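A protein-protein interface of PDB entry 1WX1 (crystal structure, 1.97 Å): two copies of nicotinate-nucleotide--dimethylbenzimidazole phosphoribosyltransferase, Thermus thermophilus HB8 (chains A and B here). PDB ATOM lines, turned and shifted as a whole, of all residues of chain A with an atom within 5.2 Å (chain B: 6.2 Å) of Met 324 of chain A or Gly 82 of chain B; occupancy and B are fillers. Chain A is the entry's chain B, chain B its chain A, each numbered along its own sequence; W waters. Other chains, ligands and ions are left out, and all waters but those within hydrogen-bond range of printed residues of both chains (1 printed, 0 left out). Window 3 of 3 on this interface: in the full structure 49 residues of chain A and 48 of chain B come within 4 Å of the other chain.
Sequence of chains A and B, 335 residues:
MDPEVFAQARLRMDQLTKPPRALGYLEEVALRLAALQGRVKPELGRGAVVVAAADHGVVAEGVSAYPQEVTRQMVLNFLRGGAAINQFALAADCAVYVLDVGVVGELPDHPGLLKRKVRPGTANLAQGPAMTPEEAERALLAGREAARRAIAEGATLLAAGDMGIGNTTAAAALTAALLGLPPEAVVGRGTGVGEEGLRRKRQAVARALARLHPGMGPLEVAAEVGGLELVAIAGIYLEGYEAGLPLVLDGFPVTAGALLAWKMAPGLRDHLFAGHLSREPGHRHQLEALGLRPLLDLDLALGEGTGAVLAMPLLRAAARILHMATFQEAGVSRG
Along chain A the printed residues that touch a printed residue of chain B span positions 17 to 325. Among the printed residues, 12 pairs touch across the chains.
The backbone carbonyl oxygen of Ala 325 of chain A is in hydrogen-bond range of the backbone NH of Thr 17 of chain A, 3.0 Å away. The backbone carbonyl oxygen (O) of Gly 81 of chain B is in hydrogen-bond range of the side-chain amide nitrogen (NE2) of Gln 87 of chain B (2.9 Å). The backbone NH (N) of Gly 82 of chain B sits at hydrogen-bond distance from the backbone carbonyl oxygen (O) of Asn 77 of chain B (3.0 Å). N of Ala 83 of chain B is in hydrogen-bond range of OD1 of Asn 86 of chain B (3.1 Å). The guanidinium group of Arg 12 of chain A is in hydrogen-bond range of the backbone carbonyl oxygen of Met 324 of chain A (2.8 Å).
Of the printed residues of chain B, Met 324 of chain A touches Gly 82, Ala 83, Ala 84 and Gln 87. Of chain A, only Thr 17 (3.7 Å), Met 324 (3.4 Å) and Ala 325 (2.8 Å) come within 4 Å of Gly 82 of chain B. Of the printed residues of chain A, Ala 84 of chain B touches Met 324 (3.6 Å). Of the printed residues of chain A, Leu 302 of chain B touches Lys 18 (3.99 Å) and Leu 23 (3.7 Å). The nearest residue of chain B that does not touch Met 324 of chain A is Leu 302 of chain B (5.5 Å). The nearest printed residue of chain A that does not touch Gln 87 of chain B is Ile 321 of chain A (4.7 Å).
Among the printed residues, pairs that only touch across the chains: Met 324 of chain A with Gly 82 of chain B, His 323 of chain A with Gln 87 of chain B, Met 324 of chain A with Gln 87 of chain B, Thr 17 of chain A with Gly 82 of chain B, Leu 23 of chain A with Leu 302 of chain B, Met 324 of chain A with Ala 83 of chain B, Ala 325 of chain A with Asn 77 of chain B and Lys 18 of chain A with Leu 302 of chain B.
The side-chain amide oxygen (OD1) of Asn 77 of chain B lies within hydrogen-bond range of the side-chain hydroxyl (OG1) of Thr 17 of chain A. The side-chain amide oxygen (OE1) of Gln 87 of chain B sits at hydrogen-bond distance from the guanidinium group (NE) of Arg 320 of chain A (2.8 Å). The backbone NH (N) of Ala 84 of chain B sits close to the side-chain sulfur (SD) of Met 324 of chain A, 3.8 Å away. The backbone carbonyl oxygen (O) of Gly 82 of chain B sits at hydrogen-bond distance from the backbone NH (N) of Ala 325 of chain A.
No position is printed for both chains.
Water W1 lies within hydrogen-bond range of the side-chain carboxylate of Glu 304 of chain B, the backbone NH of Ala 84 of chain B and the backbone carbonyl oxygen of Thr 17 of chain A.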
ATOM      1  N   ARG A  12       9.204  -1.464   9.014  1.00  0.00           N
ATOM      2  CA  ARG A  12       9.139  -1.653  10.456  1.00  0.00           C
ATOM      3  C   ARG A  12       9.068  -3.144  10.785  1.00  0.00           C
ATOM      4  O   ARG A  12       9.775  -3.622  11.672  1.00  0.00           O
ATOM      5  CB  ARG A  12       7.928  -0.930  11.053  1.00  0.00           C
ATOM      6  CG  ARG A  12       7.896  -1.009  12.570  1.00  0.00           C
ATOM      7  CD  ARG A  12       6.757  -0.218  13.183  1.00  0.00           C
ATOM      8  NE  ARG A  12       6.768  -0.357  14.636  1.00  0.00           N
ATOM      9  CZ  ARG A  12       7.660   0.218  15.435  1.00  0.00           C
ATOM     10  NH1 ARG A  12       8.616   0.986  14.924  1.00  0.00           N
ATOM     11  NH2 ARG A  12       7.613   0.006  16.746  1.00  0.00           N
ATOM     12  N   LEU A  16      11.179  -5.479  13.673  1.00  0.00           N
ATOM     13  CA  LEU A  16      10.575  -5.872  14.944  1.00  0.00           C
ATOM     14  C   LEU A  16      11.389  -6.960  15.635  1.00  0.00           C
ATOM     15  O   LEU A  16      12.085  -7.734  14.983  1.00  0.00           O
ATOM     16  CB  LEU A  16       9.138  -6.355  14.727  1.00  0.00           C
ATOM     17  CG  LEU A  16       8.183  -5.315  14.138  1.00  0.00           C
ATOM     18  CD1 LEU A  16       6.787  -5.917  14.025  1.00  0.00           C
ATOM     19  CD2 LEU A  16       8.170  -4.067  15.018  1.00  0.00           C
ATOM     20  N   THR A  17      11.286  -7.019  16.959  1.00  0.00           N
ATOM     21  CA  THR A  17      12.033  -7.994  17.745  1.00  0.00           C
ATOM     22  C   THR A  17      11.487  -9.421  17.699  1.00  0.00           C
ATOM     23  O   THR A  17      10.834  -9.885  18.629  1.00  0.00           O
ATOM     24  CB  THR A  17      12.134  -7.545  19.209  1.00  0.00           C
ATOM     25  OG1 THR A  17      10.819  -7.298  19.729  1.00  0.00           O
ATOM     26  CG2 THR A  17      12.969  -6.267  19.307  1.00  0.00           C
ATOM     27  N   LYS A  18      11.790 -10.108  16.603  1.00  0.00           N
ATOM     28  CA  LYS A  18      11.379 -11.491  16.373  1.00  0.00           C
ATOM     29  C   LYS A  18      12.142 -11.921  15.127  1.00  0.00           C
ATOM     30  O   LYS A  18      12.484 -11.082  14.296  1.00  0.00           O
ATOM     31  CB  LYS A  18       9.881 -11.567  16.077  1.00  0.00           C
ATOM     32  CG  LYS A  18       9.499 -10.674  14.905  1.00  0.00           C
ATOM     33  CD  LYS A  18       8.217 -11.086  14.222  1.00  0.00           C
ATOM     34  CE  LYS A  18       8.057 -10.283  12.935  1.00  0.00           C
ATOM     35  NZ  LYS A  18       9.299 -10.374  12.102  1.00  0.00           N
ATOM     36  N   LEU A  23       6.292 -14.716  12.788  1.00  0.00           N
ATOM     37  CA  LEU A  23       4.866 -14.610  13.100  1.00  0.00           C
ATOM     38  C   LEU A  23       3.997 -15.038  11.912  1.00  0.00           C
ATOM     39  O   LEU A  23       2.826 -14.665  11.798  1.00  0.00           O
ATOM     40  CB  LEU A  23       4.520 -13.187  13.570  1.00  0.00           C
ATOM     41  CG  LEU A  23       5.046 -12.868  14.984  1.00  0.00           C
ATOM     42  CD1 LEU A  23       4.735 -11.429  15.370  1.00  0.00           C
ATOM     43  CD2 LEU A  23       4.419 -13.832  15.992  1.00  0.00           C
ATOM     44  N   ARG A 320      -1.756  -5.490  16.305  1.00  0.00           N
ATOM     45  CA  ARG A 320      -0.852  -5.135  17.398  1.00  0.00           C
ATOM     46  C   ARG A 320       0.600  -5.540  17.150  1.00  0.00           C
ATOM     47  O   ARG A 320       1.500  -5.065  17.836  1.00  0.00           O
ATOM     48  CB  ARG A 320      -1.330  -5.752  18.719  1.00  0.00           C
ATOM     49  CG  ARG A 320      -2.583  -5.113  19.313  1.00  0.00           C
ATOM     50  CD  ARG A 320      -2.414  -3.614  19.610  1.00  0.00           C
ATOM     51  NE  ARG A 320      -1.300  -3.318  20.514  1.00  0.00           N
ATOM     52  CZ  ARG A 320      -1.162  -2.174  21.181  1.00  0.00           C
ATOM     53  NH1 ARG A 320      -2.068  -1.212  21.060  1.00  0.00           N
ATOM     54  NH2 ARG A 320      -0.108  -1.982  21.964  1.00  0.00           N
ATOM     55  N   ILE A 321       0.835  -6.421  16.182  1.00  0.00           N
ATOM     56  CA  ILE A 321       2.200  -6.848  15.877  1.00  0.00           C
ATOM     57  C   ILE A 321       3.101  -5.644  15.593  1.00  0.00           C
ATOM     58  O   ILE A 321       4.227  -5.567  16.087  1.00  0.00           O
ATOM     59  CB  ILE A 321       2.239  -7.800  14.649  1.00  0.00           C
ATOM     60  CG1 ILE A 321       1.567  -9.131  14.997  1.00  0.00           C
ATOM     61  CG2 ILE A 321       3.687  -8.020  14.195  1.00  0.00           C
ATOM     62  CD1 ILE A 321       1.522 -10.131  13.839  1.00  0.00           C
ATOM     63  N   LEU A 322       2.602  -4.701  14.802  1.00  0.00           N
ATOM     64  CA  LEU A 322       3.387  -3.517  14.460  1.00  0.00           C
ATOM     65  C   LEU A 322       3.610  -2.579  15.641  1.00  0.00           C
ATOM     66  O   LEU A 322       4.340  -1.595  15.523  1.00  0.00           O
ATOM     67  CB  LEU A 322       2.723  -2.772  13.297  1.00  0.00           C
ATOM     68  CG  LEU A 322       2.911  -3.509  11.967  1.00  0.00           C
ATOM     69  CD1 LEU A 322       1.822  -3.134  10.982  1.00  0.00           C
ATOM     70  CD2 LEU A 322       4.293  -3.189  11.412  1.00  0.00           C
ATOM     71  N   HIS A 323       2.980  -2.885  16.774  1.00  0.00           N
ATOM     72  CA  HIS A 323       3.140  -2.087  17.989  1.00  0.00           C
ATOM     73  C   HIS A 323       4.325  -2.635  18.794  1.00  0.00           C
ATOM     74  O   HIS A 323       4.718  -2.063  19.814  1.00  0.00           O
ATOM     75  CB  HIS A 323       1.862  -2.127  18.834  1.00  0.00           C
ATOM     76  CG  HIS A 323       0.736  -1.313  18.271  1.00  0.00           C
ATOM     77  ND1 HIS A 323       0.368  -0.094  18.787  1.00  0.00           N
ATOM     78  CD2 HIS A 323      -0.093  -1.546  17.221  1.00  0.00           C
ATOM     79  CE1 HIS A 323      -0.643   0.397  18.084  1.00  0.00           C
ATOM     80  NE2 HIS A 323      -0.937  -0.469  17.131  1.00  0.00           N
ATOM     81  N   MET A 324       4.886  -3.750  18.334  1.00  0.00           N
ATOM     82  CA  MET A 324       6.044  -4.347  18.993  1.00  0.00           C
ATOM     83  C   MET A 324       7.211  -3.381  18.852  1.00  0.00           C
ATOM     84  O   MET A 324       7.184  -2.475  18.017  1.00  0.00           O
ATOM     85  CB  MET A 324       6.447  -5.661  18.319  1.00  0.00           C
ATOM     86  CG  MET A 324       5.588  -6.864  18.649  1.00  0.00           C
ATOM     87  SD  MET A 324       6.073  -8.258  17.628  1.00  0.00           S
ATOM     88  CE  MET A 324       7.825  -8.467  18.120  1.00  0.00           C
ATOM     89  N   ALA A 325       8.246  -3.590  19.654  1.00  0.00           N
ATOM     90  CA  ALA A 325       9.422  -2.738  19.587  1.00  0.00           C
ATOM     91  C   ALA A 325      10.354  -3.271  18.508  1.00  0.00           C
ATOM     92  O   ALA A 325      10.331  -4.458  18.183  1.00  0.00           O
ATOM     93  CB  ALA A 325      10.141  -2.729  20.929  1.00  0.00           C
ATOM     94  N   THR A 326      11.159  -2.387  17.938  1.00  0.00           N
ATOM     95  CA  THR A 326      12.122  -2.797  16.930  1.00  0.00           C
ATOM     96  C   THR A 326      13.398  -3.131  17.696  1.00  0.00           C
ATOM     97  O   THR A 326      13.523  -2.802  18.876  1.00  0.00           O
ATOM     98  CB  THR A 326      12.424  -1.656  15.940  1.00  0.00           C
ATOM     99  OG1 THR A 326      12.869  -0.505  16.666  1.00  0.00           O
ATOM    100  CG2 THR A 326      11.183  -1.300  15.132  1.00  0.00           C
ATOM    101  N   GLU A 329      14.803   0.068  19.064  1.00  0.00           N
ATOM    102  CA  GLU A 329      14.012   0.637  20.149  1.00  0.00           C
ATOM    103  C   GLU A 329      14.171  -0.132  21.459  1.00  0.00           C
ATOM    104  O   GLU A 329      14.267   0.466  22.530  1.00  0.00           O
ATOM    105  CB  GLU A 329      12.525   0.672  19.764  1.00  0.00           C
ATOM    106  CG  GLU A 329      12.183   1.626  18.620  1.00  0.00           C
ATOM    107  CD  GLU A 329      10.786   1.394  18.049  1.00  0.00           C
ATOM    108  OE1 GLU A 329      10.394   2.132  17.117  1.00  0.00           O
ATOM    109  OE2 GLU A 329      10.081   0.475  18.524  1.00  0.00           O
ATOM    110  N   LEU B  76      13.836  -8.147  29.172  1.00  0.00           N
ATOM    111  CA  LEU B  76      13.636  -6.726  29.419  1.00  0.00           C
ATOM    112  C   LEU B  76      12.543  -6.209  28.480  1.00  0.00           C
ATOM    113  O   LEU B  76      11.722  -5.387  28.871  1.00  0.00           O
ATOM    114  CB  LEU B  76      14.942  -5.959  29.194  1.00  0.00           C
ATOM    115  CG  LEU B  76      16.023  -6.238  30.245  1.00  0.00           C
ATOM    116  CD1 LEU B  76      17.316  -5.534  29.848  1.00  0.00           C
ATOM    117  CD2 LEU B  76      15.552  -5.759  31.611  1.00  0.00           C
ATOM    118  N   ASN B  77      12.538  -6.708  27.246  1.00  0.00           N
ATOM    119  CA  ASN B  77      11.538  -6.308  26.256  1.00  0.00           C
ATOM    120  C   ASN B  77      10.155  -6.698  26.793  1.00  0.00           C
ATOM    121  O   ASN B  77       9.205  -5.920  26.685  1.00  0.00           O
ATOM    122  CB  ASN B  77      11.815  -7.017  24.918  1.00  0.00           C
ATOM    123  CG  ASN B  77      11.104  -6.361  23.730  1.00  0.00           C
ATOM    124  OD1 ASN B  77      11.033  -6.945  22.638  1.00  0.00           O
ATOM    125  ND2 ASN B  77      10.594  -5.152  23.928  1.00  0.00           N
ATOM    126  N   PHE B  78      10.051  -7.899  27.372  1.00  0.00           N
ATOM    127  CA  PHE B  78       8.788  -8.379  27.950  1.00  0.00           C
ATOM    128  C   PHE B  78       8.319  -7.416  29.036  1.00  0.00           C
ATOM    129  O   PHE B  78       7.146  -7.052  29.090  1.00  0.00           O
ATOM    130  CB  PHE B  78       8.949  -9.757  28.617  1.00  0.00           C
ATOM    131  CG  PHE B  78       9.278 -10.883  27.671  1.00  0.00           C
ATOM    132  CD1 PHE B  78       9.964 -12.008  28.134  1.00  0.00           C
ATOM    133  CD2 PHE B  78       8.928 -10.818  26.326  1.00  0.00           C
ATOM    134  CE1 PHE B  78      10.290 -13.055  27.272  1.00  0.00           C
ATOM    135  CE2 PHE B  78       9.248 -11.861  25.455  1.00  0.00           C
ATOM    136  CZ  PHE B  78       9.939 -12.976  25.930  1.00  0.00           C
ATOM    137  N   LEU B  79       9.240  -7.020  29.911  1.00  0.00           N
ATOM    138  CA  LEU B  79       8.902  -6.121  31.009  1.00  0.00           C
ATOM    139  C   LEU B  79       8.540  -4.717  30.536  1.00  0.00           C
ATOM    140  O   LEU B  79       7.885  -3.963  31.254  1.00  0.00           O
ATOM    141  CB  LEU B  79      10.060  -6.052  32.013  1.00  0.00           C
ATOM    142  CG  LEU B  79      10.481  -7.394  32.629  1.00  0.00           C
ATOM    143  CD1 LEU B  79      11.609  -7.161  33.633  1.00  0.00           C
ATOM    144  CD2 LEU B  79       9.286  -8.058  33.311  1.00  0.00           C
ATOM    145  N   ARG B  80       8.965  -4.366  29.331  1.00  0.00           N
ATOM    146  CA  ARG B  80       8.661  -3.049  28.796  1.00  0.00           C
ATOM    147  C   ARG B  80       7.509  -3.103  27.799  1.00  0.00           C
ATOM    148  O   ARG B  80       7.144  -2.091  27.205  1.00  0.00           O
ATOM    149  CB  ARG B  80       9.922  -2.447  28.179  1.00  0.00           C
ATOM    150  CG  ARG B  80      10.939  -2.097  29.258  1.00  0.00           C
ATOM    151  CD  ARG B  80      12.355  -1.921  28.734  1.00  0.00           C
ATOM    152  NE  ARG B  80      13.274  -1.693  29.847  1.00  0.00           N
ATOM    153  CZ  ARG B  80      14.595  -1.605  29.730  1.00  0.00           C
ATOM    154  NH1 ARG B  80      15.171  -1.728  28.541  1.00  0.00           N
ATOM    155  NH2 ARG B  80      15.339  -1.388  30.808  1.00  0.00           N
ATOM    156  N   GLY B  81       6.945  -4.300  27.636  1.00  0.00           N
ATOM    157  CA  GLY B  81       5.806  -4.503  26.757  1.00  0.00           C
ATOM    158  C   GLY B  81       6.011  -4.419  25.259  1.00  0.00           C
ATOM    159  O   GLY B  81       5.045  -4.198  24.525  1.00  0.00           O
ATOM    160  N   GLY B  82       7.240  -4.622  24.793  1.00  0.00           N
ATOM    161  CA  GLY B  82       7.500  -4.532  23.367  1.00  0.00           C
ATOM    162  C   GLY B  82       7.609  -5.833  22.586  1.00  0.00           C
ATOM    163  O   GLY B  82       7.911  -5.802  21.392  1.00  0.00           O
ATOM    164  N   ALA B  83       7.367  -6.970  23.233  1.00  0.00           N
ATOM    165  CA  ALA B  83       7.461  -8.259  22.549  1.00  0.00           C
ATOM    166  C   ALA B  83       6.128  -8.716  21.967  1.00  0.00           C
ATOM    167  O   ALA B  83       5.069  -8.182  22.302  1.00  0.00           O
ATOM    168  CB  ALA B  83       8.000  -9.324  23.499  1.00  0.00           C
ATOM    169  N   ALA B  84       6.187  -9.713  21.090  1.00  0.00           N
ATOM    170  CA  ALA B  84       4.983 -10.240  20.465  1.00  0.00           C
ATOM    171  C   ALA B  84       4.002 -10.722  21.529  1.00  0.00           C
ATOM    172  O   ALA B  84       2.798 -10.457  21.449  1.00  0.00           O
ATOM    173  CB  ALA B  84       5.343 -11.391  19.519  1.00  0.00           C
ATOM    174  N   ILE B  85       4.515 -11.421  22.537  1.00  0.00           N
ATOM    175  CA  ILE B  85       3.654 -11.940  23.590  1.00  0.00           C
ATOM    176  C   ILE B  85       2.868 -10.836  24.298  1.00  0.00           C
ATOM    177  O   ILE B  85       1.694 -11.020  24.618  1.00  0.00           O
ATOM    178  CB  ILE B  85       4.461 -12.773  24.634  1.00  0.00           C
ATOM    179  CG1 ILE B  85       3.491 -13.465  25.598  1.00  0.00           C
ATOM    180  CG2 ILE B  85       5.432 -11.884  25.399  1.00  0.00           C
ATOM    181  CD1 ILE B  85       2.530 -14.420  24.908  1.00  0.00           C
ATOM    182  N   ASN B  86       3.495  -9.688  24.537  1.00  0.00           N
ATOM    183  CA  ASN B  86       2.786  -8.595  25.193  1.00  0.00           C
ATOM    184  C   ASN B  86       1.629  -8.108  24.329  1.00  0.00           C
ATOM    185  O   ASN B  86       0.549  -7.805  24.839  1.00  0.00           O
ATOM    186  CB  ASN B  86       3.708  -7.402  25.460  1.00  0.00           C
ATOM    187  CG  ASN B  86       4.880  -7.755  26.340  1.00  0.00           C
ATOM    188  OD1 ASN B  86       5.983  -7.973  25.850  1.00  0.00           O
ATOM    189  ND2 ASN B  86       4.644  -7.826  27.649  1.00  0.00           N
ATOM    190  N   GLN B  87       1.867  -8.021  23.022  1.00  0.00           N
ATOM    191  CA  GLN B  87       0.850  -7.547  22.090  1.00  0.00           C
ATOM    192  C   GLN B  87      -0.325  -8.511  21.978  1.00  0.00           C
ATOM    193  O   GLN B  87      -1.485  -8.090  21.971  1.00  0.00           O
ATOM    194  CB  GLN B  87       1.466  -7.322  20.706  1.00  0.00           C
ATOM    195  CG  GLN B  87       2.597  -6.301  20.681  1.00  0.00           C
ATOM    196  CD  GLN B  87       2.266  -5.031  21.452  1.00  0.00           C
ATOM    197  OE1 GLN B  87       1.187  -4.458  21.301  1.00  0.00           O
ATOM    198  NE2 GLN B  87       3.203  -4.583  22.281  1.00  0.00           N
ATOM    199  N   LEU B 302       7.752 -18.421  16.636  1.00  0.00           N
ATOM    200  CA  LEU B 302       8.339 -17.508  17.612  1.00  0.00           C
ATOM    201  C   LEU B 302       8.473 -18.017  19.049  1.00  0.00           C
ATOM    202  O   LEU B 302       9.537 -17.880  19.654  1.00  0.00           O
ATOM    203  CB  LEU B 302       7.558 -16.192  17.619  1.00  0.00           C
ATOM    204  CG  LEU B 302       8.021 -15.139  18.625  1.00  0.00           C
ATOM    205  CD1 LEU B 302       9.482 -14.796  18.383  1.00  0.00           C
ATOM    206  CD2 LEU B 302       7.152 -13.910  18.498  1.00  0.00           C
ATOM    207  N   GLU B 304       7.545 -17.877  23.112  1.00  0.00           N
ATOM    208  CA  GLU B 304       7.138 -16.859  24.089  1.00  0.00           C
ATOM    209  C   GLU B 304       5.732 -17.119  24.639  1.00  0.00           C
ATOM    210  O   GLU B 304       5.266 -16.390  25.510  1.00  0.00           O
ATOM    211  CB  GLU B 304       7.129 -15.456  23.457  1.00  0.00           C
ATOM    212  CG  GLU B 304       8.456 -14.933  22.945  1.00  0.00           C
ATOM    213  CD  GLU B 304       8.323 -13.560  22.280  1.00  0.00           C
ATOM    214  OE1 GLU B 304       7.304 -12.861  22.509  1.00  0.00           O
ATOM    215  OE2 GLU B 304       9.246 -13.172  21.536  1.00  0.00           O
HETATM  216  O   HOH W   1       8.700 -10.770  20.347  1.00  0.00           O
